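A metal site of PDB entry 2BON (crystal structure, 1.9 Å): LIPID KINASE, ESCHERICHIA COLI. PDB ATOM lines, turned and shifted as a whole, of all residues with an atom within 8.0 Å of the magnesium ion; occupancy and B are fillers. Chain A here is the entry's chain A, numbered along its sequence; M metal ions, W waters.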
ATOM      1  N   ASP A 150      15.610 -13.227   3.910  1.00  0.00           N
ATOM      2  CA  ASP A 150      16.868 -12.496   3.865  1.00  0.00           C
ATOM      3  C   ASP A 150      18.020 -13.445   3.925  1.00  0.00           C
ATOM      4  O   ASP A 150      17.878 -14.560   4.383  1.00  0.00           O
ATOM      5  CB  ASP A 150      16.994 -11.575   5.061  1.00  0.00           C
ATOM      6  CG  ASP A 150      15.821 -10.594   5.190  1.00  0.00           C
ATOM      7  OD1 ASP A 150      15.278 -10.243   4.127  1.00  0.00           O
ATOM      8  OD2 ASP A 150      15.452 -10.215   6.343  1.00  0.00           O
ATOM      9  N   GLY A 224      22.343 -12.389  14.161  1.00  0.00           N
ATOM     10  CA  GLY A 224      21.497 -13.396  13.576  1.00  0.00           C
ATOM     11  C   GLY A 224      20.534 -13.020  12.498  1.00  0.00           C
ATOM     12  O   GLY A 224      19.748 -12.063  12.660  1.00  0.00           O
ATOM     13  N   ASN A 225      20.546 -13.796  11.398  1.00  0.00           N
ATOM     14  CA  ASN A 225      19.374 -13.832  10.529  1.00  0.00           C
ATOM     15  C   ASN A 225      18.343 -14.735  11.177  1.00  0.00           C
ATOM     16  O   ASN A 225      17.186 -14.331  11.401  1.00  0.00           O
ATOM     17  CB  ASN A 225      19.717 -14.319   9.093  1.00  0.00           C
ATOM     18  CG  ASN A 225      18.592 -14.124   8.143  1.00  0.00           C
ATOM     19  OD1 ASN A 225      17.858 -13.166   8.273  1.00  0.00           O
ATOM     20  ND2 ASN A 225      18.422 -15.008   7.176  1.00  0.00           N
ATOM     21  N   GLY A 226      18.734 -16.007  11.419  1.00  0.00           N
ATOM     22  CA  GLY A 226      17.946 -16.917  12.274  1.00  0.00           C
ATOM     23  C   GLY A 226      18.210 -16.710  13.769  1.00  0.00           C
ATOM     24  O   GLY A 226      18.829 -15.732  14.161  1.00  0.00           O
ATOM     25  N   ASN A 238      14.662 -13.307  19.232  1.00  0.00           N
ATOM     26  CA  ASN A 238      13.677 -12.449  18.601  1.00  0.00           C
ATOM     27  C   ASN A 238      13.852 -12.299  17.073  1.00  0.00           C
ATOM     28  O   ASN A 238      13.126 -11.526  16.427  1.00  0.00           O
ATOM     29  CB  ASN A 238      13.650 -11.078  19.310  1.00  0.00           C
ATOM     30  CG  ASN A 238      12.598 -10.989  20.398  1.00  0.00           C
ATOM     31  OD1 ASN A 238      11.819 -11.917  20.680  1.00  0.00           O
ATOM     32  ND2 ASN A 238      12.514  -9.807  20.995  1.00  0.00           N
ATOM     33  N   ALA A 239      14.783 -13.068  16.498  1.00  0.00           N
ATOM     34  CA  ALA A 239      15.073 -13.013  15.049  1.00  0.00           C
ATOM     35  C   ALA A 239      13.873 -13.359  14.196  1.00  0.00           C
ATOM     36  O   ALA A 239      13.067 -14.241  14.528  1.00  0.00           O
ATOM     37  CB  ALA A 239      16.259 -13.929  14.702  1.00  0.00           C
ATOM     38  N   LEU A 240      13.718 -12.604  13.111  1.00  0.00           N
ATOM     39  CA  LEU A 240      12.792 -12.969  12.025  1.00  0.00           C
ATOM     40  C   LEU A 240      13.665 -12.968  10.757  1.00  0.00           C
ATOM     41  O   LEU A 240      14.429 -12.027  10.552  1.00  0.00           O
ATOM     42  CB  LEU A 240      11.669 -11.935  11.897  1.00  0.00           C
ATOM     43  CG  LEU A 240      10.659 -11.840  13.047  1.00  0.00           C
ATOM     44  CD1 LEU A 240       9.784 -10.588  12.939  1.00  0.00           C
ATOM     45  CD2 LEU A 240       9.775 -13.081  13.079  1.00  0.00           C
ATOM     46  N   ILE A 241      13.517 -13.984   9.914  1.00  0.00           N
ATOM     47  CA  ILE A 241      14.331 -14.104   8.692  1.00  0.00           C
ATOM     48  C   ILE A 241      13.852 -13.297   7.460  1.00  0.00           C
ATOM     49  O   ILE A 241      14.488 -13.341   6.411  1.00  0.00           O
ATOM     50  CB  ILE A 241      14.513 -15.581   8.261  1.00  0.00           C
ATOM     51  CG1 ILE A 241      13.158 -16.270   8.053  1.00  0.00           C
ATOM     52  CG2 ILE A 241      15.224 -16.326   9.327  1.00  0.00           C
ATOM     53  CD1 ILE A 241      13.262 -17.714   7.574  1.00  0.00           C
ATOM     54  N   ASN A 242      12.737 -12.572   7.568  1.00  0.00           N
ATOM     55  CA  ASN A 242      12.268 -11.787   6.426  1.00  0.00           C
ATOM     56  C   ASN A 242      11.789 -10.375   6.831  1.00  0.00           C
ATOM     57  O   ASN A 242      10.856  -9.863   6.250  1.00  0.00           O
ATOM     58  CB  ASN A 242      11.172 -12.579   5.690  1.00  0.00           C
ATOM     59  CG  ASN A 242       9.913 -12.708   6.503  1.00  0.00           C
ATOM     60  OD1 ASN A 242       9.956 -12.687   7.741  1.00  0.00           O
ATOM     61  ND2 ASN A 242       8.783 -12.816   5.838  1.00  0.00           N
ATOM     62  N   ASP A 243      12.453  -9.758   7.820  1.00  0.00           N
ATOM     63  CA  ASP A 243      12.093  -8.400   8.275  1.00  0.00           C
ATOM     64  C   ASP A 243      13.091  -7.354   7.825  1.00  0.00           C
ATOM     65  O   ASP A 243      12.976  -6.157   8.155  1.00  0.00           O
ATOM     66  CB  ASP A 243      11.851  -8.355   9.796  1.00  0.00           C
ATOM     67  CG  ASP A 243      13.071  -8.713  10.627  1.00  0.00           C
ATOM     68  OD1 ASP A 243      13.023  -8.462  11.846  1.00  0.00           O
ATOM     69  OD2 ASP A 243      14.086  -9.228  10.111  1.00  0.00           O
ATOM     70  N   GLY A 244      14.099  -7.782   7.081  1.00  0.00           N
ATOM     71  CA  GLY A 244      15.158  -6.861   6.615  1.00  0.00           C
ATOM     72  C   GLY A 244      16.129  -6.502   7.678  1.00  0.00           C
ATOM     73  O   GLY A 244      16.923  -5.579   7.525  1.00  0.00           O
ATOM     74  N   LEU A 245      16.106  -7.241   8.784  1.00  0.00           N
ATOM     75  CA  LEU A 245      16.854  -6.882   9.994  1.00  0.00           C
ATOM     76  C   LEU A 245      17.648  -7.989  10.659  1.00  0.00           C
ATOM     77  O   LEU A 245      17.104  -9.046  10.967  1.00  0.00           O
ATOM     78  CB  LEU A 245      15.919  -6.221  11.024  1.00  0.00           C
ATOM     79  CG  LEU A 245      15.227  -4.927  10.617  1.00  0.00           C
ATOM     80  CD1 LEU A 245      13.969  -4.624  11.500  1.00  0.00           C
ATOM     81  CD2 LEU A 245      16.152  -3.761  10.598  1.00  0.00           C
ATOM     82  N   LEU A 246      18.930  -7.710  10.924  1.00  0.00           N
ATOM     83  CA  LEU A 246      19.798  -8.564  11.750  1.00  0.00           C
ATOM     84  C   LEU A 246      19.523  -8.276  13.223  1.00  0.00           C
ATOM     85  O   LEU A 246      19.366  -7.135  13.581  1.00  0.00           O
ATOM     86  CB  LEU A 246      21.279  -8.185  11.516  1.00  0.00           C
ATOM     87  CG  LEU A 246      21.816  -8.721  10.176  1.00  0.00           C
ATOM     88  CD1 LEU A 246      23.123  -8.016   9.839  1.00  0.00           C
ATOM     89  CD2 LEU A 246      21.953 -10.263  10.094  1.00  0.00           C
ATOM     90  N   GLN A 247      19.449  -9.331  14.034  1.00  0.00           N
ATOM     91  CA  GLN A 247      19.424  -9.185  15.480  1.00  0.00           C
ATOM     92  C   GLN A 247      20.844  -9.165  15.942  1.00  0.00           C
ATOM     93  O   GLN A 247      21.731  -9.851  15.382  1.00  0.00           O
ATOM     94  CB  GLN A 247      18.683 -10.353  16.202  1.00  0.00           C
ATOM     95  CG  GLN A 247      17.297 -10.590  15.787  1.00  0.00           C
ATOM     96  CD  GLN A 247      16.422  -9.385  15.938  1.00  0.00           C
ATOM     97  OE1 GLN A 247      15.855  -8.915  14.970  1.00  0.00           O
ATOM     98  NE2 GLN A 247      16.295  -8.882  17.146  1.00  0.00           N
ATOM     99  N   ALA A 277      18.886  -4.230  16.703  1.00  0.00           N
ATOM    100  CA  ALA A 277      18.341  -4.725  15.422  1.00  0.00           C
ATOM    101  C   ALA A 277      18.616  -3.641  14.371  1.00  0.00           C
ATOM    102  O   ALA A 277      18.354  -2.458  14.578  1.00  0.00           O
ATOM    103  CB  ALA A 277      16.818  -5.057  15.541  1.00  0.00           C
ATOM    104  N   SER A 278      19.219  -4.038  13.263  1.00  0.00           N
ATOM    105  CA  SER A 278      19.702  -3.099  12.271  1.00  0.00           C
ATOM    106  C   SER A 278      19.814  -3.866  10.941  1.00  0.00           C
ATOM    107  O   SER A 278      19.985  -5.083  10.950  1.00  0.00           O
ATOM    108  CB  SER A 278      21.072  -2.575  12.701  1.00  0.00           C
ATOM    109  OG  SER A 278      21.616  -1.707  11.730  1.00  0.00           O
ATOM    110  N   ILE A 307      22.420  -7.128   5.959  1.00  0.00           N
ATOM    111  CA  ILE A 307      21.321  -7.957   5.442  1.00  0.00           C
ATOM    112  C   ILE A 307      21.246  -7.829   3.910  1.00  0.00           C
ATOM    113  O   ILE A 307      21.508  -6.747   3.378  1.00  0.00           O
ATOM    114  CB  ILE A 307      19.997  -7.495   6.143  1.00  0.00           C
ATOM    115  CG1 ILE A 307      18.964  -8.603   6.223  1.00  0.00           C
ATOM    116  CG2 ILE A 307      19.542  -6.153   5.598  1.00  0.00           C
ATOM    117  CD1 ILE A 307      19.376  -9.651   7.342  1.00  0.00           C
ATOM    118  N   LEU A 322       9.856 -18.112  12.350  1.00  0.00           N
ATOM    119  CA  LEU A 322      10.796 -17.023  12.000  1.00  0.00           C
ATOM    120  C   LEU A 322      10.289 -16.114  10.890  1.00  0.00           C
ATOM    121  O   LEU A 322      10.974 -15.197  10.498  1.00  0.00           O
ATOM    122  CB  LEU A 322      12.180 -17.570  11.606  1.00  0.00           C
ATOM    123  CG  LEU A 322      12.964 -18.421  12.608  1.00  0.00           C
ATOM    124  CD1 LEU A 322      14.480 -18.485  12.282  1.00  0.00           C
ATOM    125  CD2 LEU A 322      12.731 -17.996  14.037  1.00  0.00           C
HETATM  126 MG    MG M   1      15.698 -10.391  10.775  1.00  0.00          MG
HETATM  127  O   HOH W   1      16.377 -10.906   8.752  1.00  0.00           O
HETATM  128  O   HOH W   2      15.077 -10.017  12.876  1.00  0.00           O
HETATM  129  O   HOH W   3      17.166 -11.777  11.655  1.00  0.00           O
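The backbone NH (N) of Asp 243 lies within hydrogen-bond range of the side-chain carboxylate (OD2) of Asp 150.
Within 4 Å of the magnesium ion: Leu 240, Asp 243 and Leu 245. The nearest printed residue that does not touch the magnesium ion is Leu 246 (4.2 Å).
The magnesium ion is bound by O of Leu 245, O of Leu 240, OD2 of Asp 243, water W1, water W3 and water W2. The magnesium ion has six donor atoms within binding distance.
Water W1 bridges the side-chain carboxylate of Asp 150 and the side-chain amide oxygen of Asn 225. Water W2 lies within hydrogen-bond range of the side-chain amide oxygen of Gln 247 (2.5 Å), the side-chain carboxylate of Asp 243 (2.8 Å) and the backbone NH of Leu 240 (2.9 Å).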
